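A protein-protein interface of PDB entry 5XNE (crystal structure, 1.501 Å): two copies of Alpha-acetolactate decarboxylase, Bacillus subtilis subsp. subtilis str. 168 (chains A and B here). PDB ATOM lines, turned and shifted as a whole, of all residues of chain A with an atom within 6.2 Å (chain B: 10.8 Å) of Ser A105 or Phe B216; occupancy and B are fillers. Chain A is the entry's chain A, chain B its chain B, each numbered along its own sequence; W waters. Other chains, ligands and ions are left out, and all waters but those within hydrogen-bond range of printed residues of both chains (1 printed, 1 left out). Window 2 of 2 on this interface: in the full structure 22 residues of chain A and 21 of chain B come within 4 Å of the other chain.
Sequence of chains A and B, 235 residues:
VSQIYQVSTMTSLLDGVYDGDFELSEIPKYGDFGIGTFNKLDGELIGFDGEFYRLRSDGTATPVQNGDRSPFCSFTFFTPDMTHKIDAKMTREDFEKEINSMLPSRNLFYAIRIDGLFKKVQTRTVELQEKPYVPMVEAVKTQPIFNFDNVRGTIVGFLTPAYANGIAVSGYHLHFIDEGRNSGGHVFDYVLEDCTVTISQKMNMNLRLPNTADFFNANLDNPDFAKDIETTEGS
Among the printed residues, merely in contact across the chains: Asn A107 with Leu B209 (3.5 Å), Asn A107 with Leu B220 (3.4 Å), Leu A108 with Leu B209 (3.6 Å), Leu A108 with Phe B215 (3.97 Å), Leu A108 with Phe B216 (3.6 Å), Phe A109 with Leu B209 (3.9 Å), Met A203 with Arg B208 (3.7 Å), Met A203 with Pro B210 (3.4 Å) and Met A203 with Phe B216 (3.8 Å).
Water W1 lies within hydrogen-bond range of the side-chain amide oxygen of Asn A107 (2.7 Å), the backbone NH of Leu B220 (2.9 Å) and the backbone carbonyl oxygen of Ala B218 (3.3 Å).
The backbone NH (N) of Ser B8 lies within hydrogen-bond range of the backbone carbonyl oxygen (O) of Arg B208 (2.9 Å).
The backbone NH of Phe B215 sits at hydrogen-bond distance from the side-chain hydroxyl of Thr B212 (3.0 Å).
N of Asn A107 is in hydrogen-bond range of OG of Ser A105.
The side-chain hydroxyl (OH) of Tyr A110 is in hydrogen-bond range of the backbone carbonyl oxygen (O) of Ser A105.
The side-chain amide nitrogen of Gln A201 lies within hydrogen-bond range of the side-chain sulfur of Met A203 (3.8 Å).
No position is printed for both chains.
Met A102 touches none of the printed residues of chain B.
No residue of chain B comes within 4 Å of Pro A104.
Of chain B, only Phe B216 (2.7 Å) comes within 4 Å of Ser A105.
Asn A107 touches just these residues of chain B: Leu B209, Phe B215, Phe B216, Ala B218 and Leu B220.
Printed residues of chain B within 4 Å of Leu A108: Leu B209 (3.6 Å), Phe B215 (3.97 Å) and Phe B216 (3.6 Å).
Of the printed residues of chain B, Phe A109 touches Leu B209 (3.9 Å).
Of the printed residues of chain A, Pro B210 touches Met A203 (3.4 Å).
Of the printed residues of chain A, Phe B215 touches Asn A107 (2.9 Å) and Leu A108 (3.97 Å).
Of chain A, only Ser A105, Asn A107, Leu A108 and Met A203 come within 4 Å of Phe B216.
Of the printed residues of chain A, Ala B218 touches Asn A107.
Printed residues of chain A within 4 Å of Leu B220: Asn A107 (3.4 Å).
Asp B221 touches none of the printed residues of chain A.
The nearest printed residue of chain A that does not touch Leu B220 is Arg A106 (6.3 Å).
Of the 25 printed residues of chain B, 7 touch a printed residue of chain A.
Hydrophobic or aromatic side chains of chain B within 4 Å of the printed part of chain A: Leu B209, Phe B215, Phe B216, Ala B218 and Leu B220.
Hydrophobic or aromatic side chains of chain A within 4 Å of the printed part of chain B: Leu A108, Phe A109 and Met A203.
Among the printed residues, 14 pairs touch across the chains.
The backbone carbonyl oxygen (O) of Met A203 is in hydrogen-bond range of the backbone NH (N) of Leu B209, 2.8 Å away.
The backbone carbonyl oxygen (O) of Phe B215 lies within hydrogen-bond range of the side-chain amide nitrogen (ND2) of Asn A107 (2.9 Å).
The backbone carbonyl oxygen (O) of Phe B216 is in hydrogen-bond range of the side-chain hydroxyl (OG) of Ser A105.
The side-chain amide nitrogen of Asn A107 lies within hydrogen-bond range of the backbone carbonyl oxygen of Phe B216 (3.4 Å).
The backbone carbonyl oxygen (O) of Ala B218 lies within hydrogen-bond range of the side-chain amide nitrogen (ND2) of Asn A107 (3.0 Å).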
ATOM      1  N   MET A 102     -35.793  -7.561 -25.937  1.00  0.00           N
ATOM      2  CA  MET A 102     -34.735  -7.330 -26.926  1.00  0.00           C
ATOM      3  C   MET A 102     -33.716  -6.272 -26.469  1.00  0.00           C
ATOM      4  O   MET A 102     -32.626  -6.150 -27.033  1.00  0.00           O
ATOM      5  CB  MET A 102     -35.377  -6.943 -28.265  1.00  0.00           C
ATOM      6  CG  MET A 102     -34.749  -5.776 -29.012  1.00  0.00           C
ATOM      7  SD  MET A 102     -35.330  -5.670 -30.717  1.00  0.00           S
ATOM      8  CE  MET A 102     -34.423  -4.232 -31.298  1.00  0.00           C
ATOM      9  N   LEU A 103     -34.068  -5.519 -25.434  1.00  0.00           N
ATOM     10  CA  LEU A 103     -33.142  -4.544 -24.863  1.00  0.00           C
ATOM     11  C   LEU A 103     -31.907  -5.245 -24.312  1.00  0.00           C
ATOM     12  O   LEU A 103     -32.027  -6.317 -23.717  1.00  0.00           O
ATOM     13  CB  LEU A 103     -33.819  -3.754 -23.752  1.00  0.00           C
ATOM     14  CG  LEU A 103     -35.127  -3.078 -24.154  1.00  0.00           C
ATOM     15  CD1 LEU A 103     -35.895  -2.739 -22.918  1.00  0.00           C
ATOM     16  CD2 LEU A 103     -34.844  -1.843 -24.974  1.00  0.00           C
ATOM     17  N   PRO A 104     -30.722  -4.644 -24.511  1.00  0.00           N
ATOM     18  CA  PRO A 104     -29.474  -5.161 -23.939  1.00  0.00           C
ATOM     19  C   PRO A 104     -29.574  -5.287 -22.420  1.00  0.00           C
ATOM     20  O   PRO A 104     -28.971  -6.177 -21.818  1.00  0.00           O
ATOM     21  CB  PRO A 104     -28.437  -4.104 -24.339  1.00  0.00           C
ATOM     22  CG  PRO A 104     -29.009  -3.453 -25.547  1.00  0.00           C
ATOM     23  CD  PRO A 104     -30.495  -3.459 -25.355  1.00  0.00           C
ATOM     24  N   SER A 105     -30.352  -4.403 -21.808  1.00  0.00           N
ATOM     25  CA  SER A 105     -30.489  -4.406 -20.357  1.00  0.00           C
ATOM     26  C   SER A 105     -31.707  -3.604 -19.906  1.00  0.00           C
ATOM     27  O   SER A 105     -31.987  -2.538 -20.449  1.00  0.00           O
ATOM     28  CB  SER A 105     -29.232  -3.830 -19.695  1.00  0.00           C
ATOM     29  OG  SER A 105     -29.415  -3.657 -18.294  1.00  0.00           O
ATOM     30  N   ARG A 106     -32.397  -4.109 -18.894  1.00  0.00           N
ATOM     31  CA  ARG A 106     -33.481  -3.366 -18.267  1.00  0.00           C
ATOM     32  C   ARG A 106     -32.976  -2.316 -17.273  1.00  0.00           C
ATOM     33  O   ARG A 106     -33.764  -1.648 -16.608  1.00  0.00           O
ATOM     34  CB  ARG A 106     -34.423  -4.329 -17.563  1.00  0.00           C
ATOM     35  CG  ARG A 106     -35.282  -5.156 -18.498  1.00  0.00           C
ATOM     36  CD  ARG A 106     -36.674  -5.001 -17.964  1.00  0.00           C
ATOM     37  NE  ARG A 106     -37.761  -5.326 -18.878  1.00  0.00           N
ATOM     38  CZ  ARG A 106     -39.029  -5.324 -18.479  1.00  0.00           C
ATOM     39  NH1 ARG A 106     -39.317  -5.003 -17.222  1.00  0.00           N
ATOM     40  NH2 ARG A 106     -40.005  -5.620 -19.313  1.00  0.00           N
ATOM     41  N   ASN A 107     -31.660  -2.166 -17.184  1.00  0.00           N
ATOM     42  CA  ASN A 107     -31.064  -1.246 -16.224  1.00  0.00           C
ATOM     43  C   ASN A 107     -30.516   0.019 -16.877  1.00  0.00           C
ATOM     44  O   ASN A 107     -29.853   0.818 -16.217  1.00  0.00           O
ATOM     45  CB  ASN A 107     -29.956  -1.958 -15.449  1.00  0.00           C
ATOM     46  CG  ASN A 107     -30.453  -3.219 -14.782  1.00  0.00           C
ATOM     47  OD1 ASN A 107     -31.598  -3.282 -14.324  1.00  0.00           O
ATOM     48  ND2 ASN A 107     -29.596  -4.239 -14.722  1.00  0.00           N
ATOM     49  N   LEU A 108     -30.782   0.179 -18.169  1.00  0.00           N
ATOM     50  CA  LEU A 108     -30.325   1.346 -18.919  1.00  0.00           C
ATOM     51  C   LEU A 108     -31.501   2.203 -19.346  1.00  0.00           C
ATOM     52  O   LEU A 108     -32.644   1.788 -19.230  1.00  0.00           O
ATOM     53  CB  LEU A 108     -29.527   0.930 -20.153  1.00  0.00           C
ATOM     54  CG  LEU A 108     -28.329   0.024 -19.883  1.00  0.00           C
ATOM     55  CD1 LEU A 108     -27.663  -0.326 -21.222  1.00  0.00           C
ATOM     56  CD2 LEU A 108     -27.355   0.691 -18.934  1.00  0.00           C
ATOM     57  N   PHE A 109     -31.213   3.406 -19.829  1.00  0.00           N
ATOM     58  CA  PHE A 109     -32.251   4.301 -20.361  1.00  0.00           C
ATOM     59  C   PHE A 109     -32.338   4.175 -21.876  1.00  0.00           C
ATOM     60  O   PHE A 109     -31.308   4.047 -22.541  1.00  0.00           O
ATOM     61  CB  PHE A 109     -31.946   5.754 -19.993  1.00  0.00           C
ATOM     62  CG  PHE A 109     -32.043   6.047 -18.518  1.00  0.00           C
ATOM     63  CD1 PHE A 109     -31.014   5.687 -17.646  1.00  0.00           C
ATOM     64  CD2 PHE A 109     -33.155   6.703 -18.004  1.00  0.00           C
ATOM     65  CE1 PHE A 109     -31.116   5.959 -16.277  1.00  0.00           C
ATOM     66  CE2 PHE A 109     -33.256   6.982 -16.640  1.00  0.00           C
ATOM     67  CZ  PHE A 109     -32.236   6.611 -15.788  1.00  0.00           C
ATOM     68  N   TYR A 110     -33.553   4.215 -22.428  1.00  0.00           N
ATOM     69  CA  TYR A 110     -33.718   4.177 -23.884  1.00  0.00           C
ATOM     70  C   TYR A 110     -34.694   5.238 -24.352  1.00  0.00           C
ATOM     71  O   TYR A 110     -35.684   5.523 -23.679  1.00  0.00           O
ATOM     72  CB  TYR A 110     -34.222   2.803 -24.368  1.00  0.00           C
ATOM     73  CG  TYR A 110     -33.334   1.662 -23.957  1.00  0.00           C
ATOM     74  CD1 TYR A 110     -33.527   1.022 -22.741  1.00  0.00           C
ATOM     75  CD2 TYR A 110     -32.287   1.246 -24.768  1.00  0.00           C
ATOM     76  CE1 TYR A 110     -32.706  -0.028 -22.338  1.00  0.00           C
ATOM     77  CE2 TYR A 110     -31.457   0.200 -24.376  1.00  0.00           C
ATOM     78  CZ  TYR A 110     -31.678  -0.426 -23.156  1.00  0.00           C
ATOM     79  OH  TYR A 110     -30.862  -1.467 -22.752  1.00  0.00           O
ATOM     80  N   LEU A 159     -37.998   4.586 -22.293  1.00  0.00           N
ATOM     81  CA  LEU A 159     -38.036   3.502 -21.312  1.00  0.00           C
ATOM     82  C   LEU A 159     -37.104   3.856 -20.165  1.00  0.00           C
ATOM     83  O   LEU A 159     -35.934   4.185 -20.370  1.00  0.00           O
ATOM     84  CB  LEU A 159     -37.634   2.158 -21.922  1.00  0.00           C
ATOM     85  CG  LEU A 159     -37.891   0.998 -20.932  1.00  0.00           C
ATOM     86  CD1 LEU A 159     -39.321   0.395 -20.976  1.00  0.00           C
ATOM     87  CD2 LEU A 159     -36.830  -0.061 -21.048  1.00  0.00           C
ATOM     88  N   GLN A 201     -29.963   3.977 -27.087  1.00  0.00           N
ATOM     89  CA  GLN A 201     -29.540   3.572 -25.749  1.00  0.00           C
ATOM     90  C   GLN A 201     -28.704   4.673 -25.099  1.00  0.00           C
ATOM     91  O   GLN A 201     -27.800   5.222 -25.726  1.00  0.00           O
ATOM     92  CB  GLN A 201     -28.736   2.261 -25.830  1.00  0.00           C
ATOM     93  CG  GLN A 201     -28.059   1.850 -24.528  1.00  0.00           C
ATOM     94  CD  GLN A 201     -27.258   0.570 -24.692  1.00  0.00           C
ATOM     95  OE1 GLN A 201     -27.793  -0.452 -25.114  1.00  0.00           O
ATOM     96  NE2 GLN A 201     -25.972   0.628 -24.377  1.00  0.00           N
ATOM     97  N   MET A 203     -26.417   5.903 -21.512  1.00  0.00           N
ATOM     98  CA  MET A 203     -25.709   5.439 -20.310  1.00  0.00           C
ATOM     99  C   MET A 203     -25.668   6.467 -19.188  1.00  0.00           C
ATOM    100  O   MET A 203     -25.079   6.219 -18.146  1.00  0.00           O
ATOM    101  CB  MET A 203     -24.264   5.049 -20.646  1.00  0.00           C
ATOM    102  CG  MET A 203     -24.125   4.008 -21.729  1.00  0.00           C
ATOM    103  SD  MET A 203     -24.952   2.482 -21.266  1.00  0.00           S
ATOM    104  CE  MET A 203     -23.760   1.762 -20.118  1.00  0.00           C
ATOM    105  N   SER B   8     -22.958   4.753 -10.949  1.00  0.00           N
ATOM    106  CA  SER B   8     -23.857   3.600 -10.789  1.00  0.00           C
ATOM    107  C   SER B   8     -24.876   3.770  -9.651  1.00  0.00           C
ATOM    108  O   SER B   8     -25.097   4.892  -9.166  1.00  0.00           O
ATOM    109  CB  SER B   8     -23.046   2.309 -10.572  1.00  0.00           C
ATOM    110  OG  SER B   8     -23.845   1.159 -10.846  1.00  0.00           O
ATOM    111  N   THR B   9     -25.512   2.671  -9.244  1.00  0.00           N
ATOM    112  CA  THR B   9     -26.617   2.755  -8.292  1.00  0.00           C
ATOM    113  C   THR B   9     -26.408   1.914  -7.047  1.00  0.00           C
ATOM    114  O   THR B   9     -25.742   0.865  -7.077  1.00  0.00           O
ATOM    115  CB  THR B   9     -27.965   2.312  -8.921  1.00  0.00           C
ATOM    116  OG1 THR B   9     -27.995   0.877  -9.036  1.00  0.00           O
ATOM    117  CG2 THR B   9     -28.165   2.956 -10.286  1.00  0.00           C
ATOM    118  N   SER B  12     -27.677  -1.651  -7.451  1.00  0.00           N
ATOM    119  CA  SER B  12     -26.747  -2.590  -8.091  1.00  0.00           C
ATOM    120  C   SER B  12     -25.757  -3.158  -7.070  1.00  0.00           C
ATOM    121  O   SER B  12     -25.447  -4.361  -7.079  1.00  0.00           O
ATOM    122  CB  SER B  12     -26.016  -1.926  -9.270  1.00  0.00           C
ATOM    123  OG  SER B  12     -25.160  -2.858  -9.938  1.00  0.00           O
ATOM    124  N   LEU B  13     -25.265  -2.310  -6.172  1.00  0.00           N
ATOM    125  CA  LEU B  13     -24.422  -2.775  -5.090  1.00  0.00           C
ATOM    126  C   LEU B  13     -25.180  -3.779  -4.196  1.00  0.00           C
ATOM    127  O   LEU B  13     -24.634  -4.829  -3.833  1.00  0.00           O
ATOM    128  CB  LEU B  13     -23.904  -1.578  -4.283  1.00  0.00           C
ATOM    129  CG  LEU B  13     -22.538  -1.683  -3.614  1.00  0.00           C
ATOM    130  CD1 LEU B  13     -21.406  -1.832  -4.620  1.00  0.00           C
ATOM    131  CD2 LEU B  13     -22.318  -0.464  -2.717  1.00  0.00           C
ATOM    132  N   ASP B  15     -27.306  -5.859  -5.060  1.00  0.00           N
ATOM    133  CA  ASP B  15     -27.439  -7.115  -5.797  1.00  0.00           C
ATOM    134  C   ASP B  15     -26.100  -7.847  -5.940  1.00  0.00           C
ATOM    135  O   ASP B  15     -26.022  -8.895  -6.588  1.00  0.00           O
ATOM    136  CB  ASP B  15     -28.045  -6.855  -7.179  1.00  0.00           C
ATOM    137  CG  ASP B  15     -28.446  -8.139  -7.895  1.00  0.00           C
ATOM    138  OD1 ASP B  15     -29.092  -8.999  -7.254  1.00  0.00           O
ATOM    139  OD2 ASP B  15     -28.095  -8.292  -9.085  1.00  0.00           O
ATOM    140  N   VAL B  17     -23.207  -6.599  -7.244  1.00  0.00           N
ATOM    141  CA  VAL B  17     -22.382  -6.189  -8.365  1.00  0.00           C
ATOM    142  C   VAL B  17     -21.277  -5.321  -7.781  1.00  0.00           C
ATOM    143  O   VAL B  17     -21.433  -4.112  -7.617  1.00  0.00           O
ATOM    144  CB  VAL B  17     -23.192  -5.438  -9.429  1.00  0.00           C
ATOM    145  CG1 VAL B  17     -22.299  -4.918 -10.544  1.00  0.00           C
ATOM    146  CG2 VAL B  17     -24.269  -6.356  -9.992  1.00  0.00           C
ATOM    147  N   TYR B  18     -20.170  -5.951  -7.424  1.00  0.00           N
ATOM    148  CA  TYR B  18     -19.099  -5.217  -6.749  1.00  0.00           C
ATOM    149  C   TYR B  18     -17.967  -4.788  -7.677  1.00  0.00           C
ATOM    150  O   TYR B  18     -17.017  -4.141  -7.239  1.00  0.00           O
ATOM    151  CB  TYR B  18     -18.526  -6.052  -5.602  1.00  0.00           C
ATOM    152  CG  TYR B  18     -19.555  -6.459  -4.573  1.00  0.00           C
ATOM    153  CD1 TYR B  18     -20.594  -5.601  -4.214  1.00  0.00           C
ATOM    154  CD2 TYR B  18     -19.503  -7.711  -3.971  1.00  0.00           C
ATOM    155  CE1 TYR B  18     -21.547  -5.976  -3.273  1.00  0.00           C
ATOM    156  CE2 TYR B  18     -20.452  -8.096  -3.036  1.00  0.00           C
ATOM    157  CZ  TYR B  18     -21.472  -7.234  -2.693  1.00  0.00           C
ATOM    158  OH  TYR B  18     -22.414  -7.614  -1.767  1.00  0.00           O
ATOM    159  N   ASP B  19     -18.057  -5.142  -8.950  1.00  0.00           N
ATOM    160  CA  ASP B  19     -17.013  -4.786  -9.904  1.00  0.00           C
ATOM    161  C   ASP B  19     -17.555  -3.774 -10.900  1.00  0.00           C
ATOM    162  O   ASP B  19     -18.451  -4.096 -11.677  1.00  0.00           O
ATOM    163  CB  ASP B  19     -16.494  -6.028 -10.644  1.00  0.00           C
ATOM    164  CG  ASP B  19     -15.664  -6.952  -9.753  1.00  0.00           C
ATOM    165  OD1 ASP B  19     -15.594  -6.732  -8.527  1.00  0.00           O
ATOM    166  OD2 ASP B  19     -15.090  -7.908 -10.301  1.00  0.00           O
ATOM    167  N   GLY B  20     -17.046  -2.546 -10.864  1.00  0.00           N
ATOM    168  CA  GLY B  20     -17.435  -1.553 -11.847  1.00  0.00           C
ATOM    169  C   GLY B  20     -16.309  -1.255 -12.819  1.00  0.00           C
ATOM    170  O   GLY B  20     -15.249  -1.890 -12.771  1.00  0.00           O
ATOM    171  N   ASP B  21     -16.533  -0.288 -13.704  1.00  0.00           N
ATOM    172  CA  ASP B  21     -15.500   0.085 -14.661  1.00  0.00           C
ATOM    173  C   ASP B  21     -15.041   1.534 -14.504  1.00  0.00           C
ATOM    174  O   ASP B  21     -14.226   2.015 -15.297  1.00  0.00           O
ATOM    175  CB  ASP B  21     -15.978  -0.179 -16.098  1.00  0.00           C
ATOM    176  CG  ASP B  21     -17.184   0.659 -16.493  1.00  0.00           C
ATOM    177  OD1 ASP B  21     -17.811   1.294 -15.616  1.00  0.00           O
ATOM    178  OD2 ASP B  21     -17.531   0.663 -17.701  1.00  0.00           O
ATOM    179  N   PRO B  71     -17.355   0.285  -8.272  1.00  0.00           N
ATOM    180  CA  PRO B  71     -18.728  -0.014  -8.691  1.00  0.00           C
ATOM    181  C   PRO B  71     -19.734   1.034  -8.232  1.00  0.00           C
ATOM    182  O   PRO B  71     -20.886   0.968  -8.659  1.00  0.00           O
ATOM    183  CB  PRO B  71     -19.020  -1.341  -7.988  1.00  0.00           C
ATOM    184  CG  PRO B  71     -18.266  -1.199  -6.674  1.00  0.00           C
ATOM    185  CD  PRO B  71     -17.001  -0.410  -7.015  1.00  0.00           C
ATOM    186  N   ARG B 208     -24.083   8.124 -14.022  1.00  0.00           N
ATOM    187  CA  ARG B 208     -23.329   7.395 -15.051  1.00  0.00           C
ATOM    188  C   ARG B 208     -23.425   5.892 -14.807  1.00  0.00           C
ATOM    189  O   ARG B 208     -23.030   5.396 -13.746  1.00  0.00           O
ATOM    190  CB  ARG B 208     -21.871   7.837 -15.041  1.00  0.00           C
ATOM    191  CG  ARG B 208     -20.932   6.960 -15.855  1.00  0.00           C
ATOM    192  CD  ARG B 208     -21.330   6.952 -17.326  1.00  0.00           C
ATOM    193  NE  ARG B 208     -20.183   6.662 -18.185  1.00  0.00           N
ATOM    194  CZ  ARG B 208     -19.659   5.452 -18.351  1.00  0.00           C
ATOM    195  NH1 ARG B 208     -20.170   4.415 -17.713  1.00  0.00           N
ATOM    196  NH2 ARG B 208     -18.613   5.284 -19.153  1.00  0.00           N
ATOM    197  N   LEU B 209     -23.966   5.166 -15.779  1.00  0.00           N
ATOM    198  CA  LEU B 209     -24.116   3.717 -15.640  1.00  0.00           C
ATOM    199  C   LEU B 209     -22.889   3.015 -16.210  1.00  0.00           C
ATOM    200  O   LEU B 209     -22.356   3.434 -17.228  1.00  0.00           O
ATOM    201  CB  LEU B 209     -25.377   3.242 -16.362  1.00  0.00           C
ATOM    202  CG  LEU B 209     -26.628   4.031 -15.956  1.00  0.00           C
ATOM    203  CD1 LEU B 209     -27.816   3.623 -16.818  1.00  0.00           C
ATOM    204  CD2 LEU B 209     -26.875   3.799 -14.480  1.00  0.00           C
ATOM    205  N   PRO B 210     -22.438   1.946 -15.540  1.00  0.00           N
ATOM    206  CA  PRO B 210     -21.232   1.259 -16.026  1.00  0.00           C
ATOM    207  C   PRO B 210     -21.483   0.441 -17.284  1.00  0.00           C
ATOM    208  O   PRO B 210     -22.581  -0.083 -17.484  1.00  0.00           O
ATOM    209  CB  PRO B 210     -20.842   0.345 -14.860  1.00  0.00           C
ATOM    210  CG  PRO B 210     -22.090   0.144 -14.070  1.00  0.00           C
ATOM    211  CD  PRO B 210     -22.985   1.350 -14.308  1.00  0.00           C
ATOM    212  N   ASN B 211     -20.454   0.338 -18.122  1.00  0.00           N
ATOM    213  CA  ASN B 211     -20.533  -0.489 -19.316  1.00  0.00           C
ATOM    214  C   ASN B 211     -19.994  -1.874 -19.008  1.00  0.00           C
ATOM    215  O   ASN B 211     -18.991  -2.301 -19.571  1.00  0.00           O
ATOM    216  CB  ASN B 211     -19.765   0.153 -20.464  1.00  0.00           C
ATOM    217  CG  ASN B 211     -20.054  -0.506 -21.786  1.00  0.00           C
ATOM    218  OD1 ASN B 211     -21.149  -1.024 -22.005  1.00  0.00           O
ATOM    219  ND2 ASN B 211     -19.078  -0.488 -22.683  1.00  0.00           N
ATOM    220  N   THR B 212     -20.645  -2.551 -18.074  1.00  0.00           N
ATOM    221  CA  THR B 212     -20.229  -3.892 -17.681  1.00  0.00           C
ATOM    222  C   THR B 212     -21.357  -4.891 -17.872  1.00  0.00           C
ATOM    223  O   THR B 212     -22.546  -4.583 -17.685  1.00  0.00           O
ATOM    224  CB  THR B 212     -19.785  -3.954 -16.224  1.00  0.00           C
ATOM    225  OG1 THR B 212     -20.914  -3.685 -15.389  1.00  0.00           O
ATOM    226  CG2 THR B 212     -18.666  -2.932 -15.950  1.00  0.00           C
ATOM    227  N   ALA B 213     -20.987  -6.110 -18.232  1.00  0.00           N
ATOM    228  CA  ALA B 213     -21.977  -7.158 -18.352  1.00  0.00           C
ATOM    229  C   ALA B 213     -22.678  -7.397 -17.008  1.00  0.00           C
ATOM    230  O   ALA B 213     -23.881  -7.648 -16.964  1.00  0.00           O
ATOM    231  CB  ALA B 213     -21.328  -8.439 -18.863  1.00  0.00           C
ATOM    232  N   ASP B 214     -21.918  -7.304 -15.913  1.00  0.00           N
ATOM    233  CA  ASP B 214     -22.470  -7.491 -14.570  1.00  0.00           C
ATOM    234  C   ASP B 214     -23.600  -6.506 -14.282  1.00  0.00           C
ATOM    235  O   ASP B 214     -24.635  -6.870 -13.730  1.00  0.00           O
ATOM    236  CB  ASP B 214     -21.385  -7.328 -13.506  1.00  0.00           C
ATOM    237  CG  ASP B 214     -20.397  -8.466 -13.501  1.00  0.00           C
ATOM    238  OD1 ASP B 214     -20.767  -9.569 -13.951  1.00  0.00           O
ATOM    239  OD2 ASP B 214     -19.251  -8.251 -13.036  1.00  0.00           O
ATOM    240  N   PHE B 215     -23.399  -5.250 -14.656  1.00  0.00           N
ATOM    241  CA  PHE B 215     -24.449  -4.271 -14.430  1.00  0.00           C
ATOM    242  C   PHE B 215     -25.609  -4.497 -15.396  1.00  0.00           C
ATOM    243  O   PHE B 215     -26.763  -4.440 -15.001  1.00  0.00           O
ATOM    244  CB  PHE B 215     -23.927  -2.843 -14.579  1.00  0.00           C
ATOM    245  CG  PHE B 215     -24.990  -1.813 -14.332  1.00  0.00           C
ATOM    246  CD1 PHE B 215     -25.331  -1.467 -13.034  1.00  0.00           C
ATOM    247  CD2 PHE B 215     -25.682  -1.234 -15.392  1.00  0.00           C
ATOM    248  CE1 PHE B 215     -26.327  -0.538 -12.787  1.00  0.00           C
ATOM    249  CE2 PHE B 215     -26.697  -0.294 -15.147  1.00  0.00           C
ATOM    250  CZ  PHE B 215     -27.014   0.043 -13.842  1.00  0.00           C
ATOM    251  N   PHE B 216     -25.303  -4.726 -16.668  1.00  0.00           N
ATOM    252  CA  PHE B 216     -26.355  -4.980 -17.663  1.00  0.00           C
ATOM    253  C   PHE B 216     -27.288  -6.122 -17.221  1.00  0.00           C
ATOM    254  O   PHE B 216     -28.518  -6.048 -17.376  1.00  0.00           O
ATOM    255  CB  PHE B 216     -25.754  -5.334 -19.024  1.00  0.00           C
ATOM    256  CG  PHE B 216     -25.323  -4.148 -19.849  1.00  0.00           C
ATOM    257  CD1 PHE B 216     -24.714  -3.041 -19.263  1.00  0.00           C
ATOM    258  CD2 PHE B 216     -25.509  -4.151 -21.226  1.00  0.00           C
ATOM    259  CE1 PHE B 216     -24.307  -1.975 -20.027  1.00  0.00           C
ATOM    260  CE2 PHE B 216     -25.101  -3.069 -22.006  1.00  0.00           C
ATOM    261  CZ  PHE B 216     -24.495  -1.983 -21.405  1.00  0.00           C
ATOM    262  N   ASN B 217     -26.692  -7.172 -16.654  1.00  0.00           N
ATOM    263  CA  ASN B 217     -27.434  -8.383 -16.300  1.00  0.00           C
ATOM    264  C   ASN B 217     -27.959  -8.415 -14.863  1.00  0.00           C
ATOM    265  O   ASN B 217     -28.631  -9.369 -14.467  1.00  0.00           O
ATOM    266  CB  ASN B 217     -26.551  -9.612 -16.544  1.00  0.00           C
ATOM    267  CG  ASN B 217     -26.213  -9.804 -18.010  1.00  0.00           C
ATOM    268  OD1 ASN B 217     -27.018  -9.498 -18.886  1.00  0.00           O
ATOM    269  ND2 ASN B 217     -25.014 -10.331 -18.285  1.00  0.00           N
ATOM    270  N   ALA B 218     -27.646  -7.391 -14.078  1.00  0.00           N
ATOM    271  CA  ALA B 218     -28.078  -7.332 -12.680  1.00  0.00           C
ATOM    272  C   ALA B 218     -29.597  -7.306 -12.527  1.00  0.00           C
ATOM    273  O   ALA B 218     -30.319  -6.770 -13.375  1.00  0.00           O
ATOM    274  CB  ALA B 218     -27.478  -6.113 -11.987  1.00  0.00           C
ATOM    275  N   ASN B 219     -30.066  -7.866 -11.414  1.00  0.00           N
ATOM    276  CA  ASN B 219     -31.477  -7.791 -11.047  1.00  0.00           C
ATOM    277  C   ASN B 219     -31.687  -6.619 -10.100  1.00  0.00           C
ATOM    278  O   ASN B 219     -31.313  -6.672  -8.928  1.00  0.00           O
ATOM    279  CB  ASN B 219     -31.940  -9.107 -10.413  1.00  0.00           C
ATOM    280  CG  ASN B 219     -33.373  -9.045  -9.909  1.00  0.00           C
ATOM    281  OD1 ASN B 219     -34.142  -8.150 -10.267  1.00  0.00           O
ATOM    282  ND2 ASN B 219     -33.738 -10.007  -9.066  1.00  0.00           N
ATOM    283  N   LEU B 220     -32.283  -5.550 -10.618  1.00  0.00           N
ATOM    284  CA  LEU B 220     -32.445  -4.329  -9.848  1.00  0.00           C
ATOM    285  C   LEU B 220     -33.908  -4.070  -9.520  1.00  0.00           C
ATOM    286  O   LEU B 220     -34.317  -2.922  -9.324  1.00  0.00           O
ATOM    287  CB  LEU B 220     -31.859  -3.140 -10.610  1.00  0.00           C
ATOM    288  CG  LEU B 220     -30.393  -3.282 -11.023  1.00  0.00           C
ATOM    289  CD1 LEU B 220     -29.862  -1.994 -11.641  1.00  0.00           C
ATOM    290  CD2 LEU B 220     -29.552  -3.678  -9.815  1.00  0.00           C
ATOM    291  N   ASP B 221     -34.699  -5.134  -9.471  1.00  0.00           N
ATOM    292  CA  ASP B 221     -36.118  -4.983  -9.163  1.00  0.00           C
ATOM    293  C   ASP B 221     -36.468  -5.587  -7.813  1.00  0.00           C
ATOM    294  O   ASP B 221     -37.382  -6.405  -7.704  1.00  0.00           O
ATOM    295  CB  ASP B 221     -36.982  -5.605 -10.261  1.00  0.00           C
ATOM    296  CG  ASP B 221     -37.044  -4.742 -11.508  1.00  0.00           C
ATOM    297  OD1 ASP B 221     -37.179  -3.499 -11.381  1.00  0.00           O
ATOM    298  OD2 ASP B 221     -36.955  -5.304 -12.623  1.00  0.00           O
HETATM  299  O   HOH W   1     -33.211  -5.214 -13.370  1.00  0.00           O
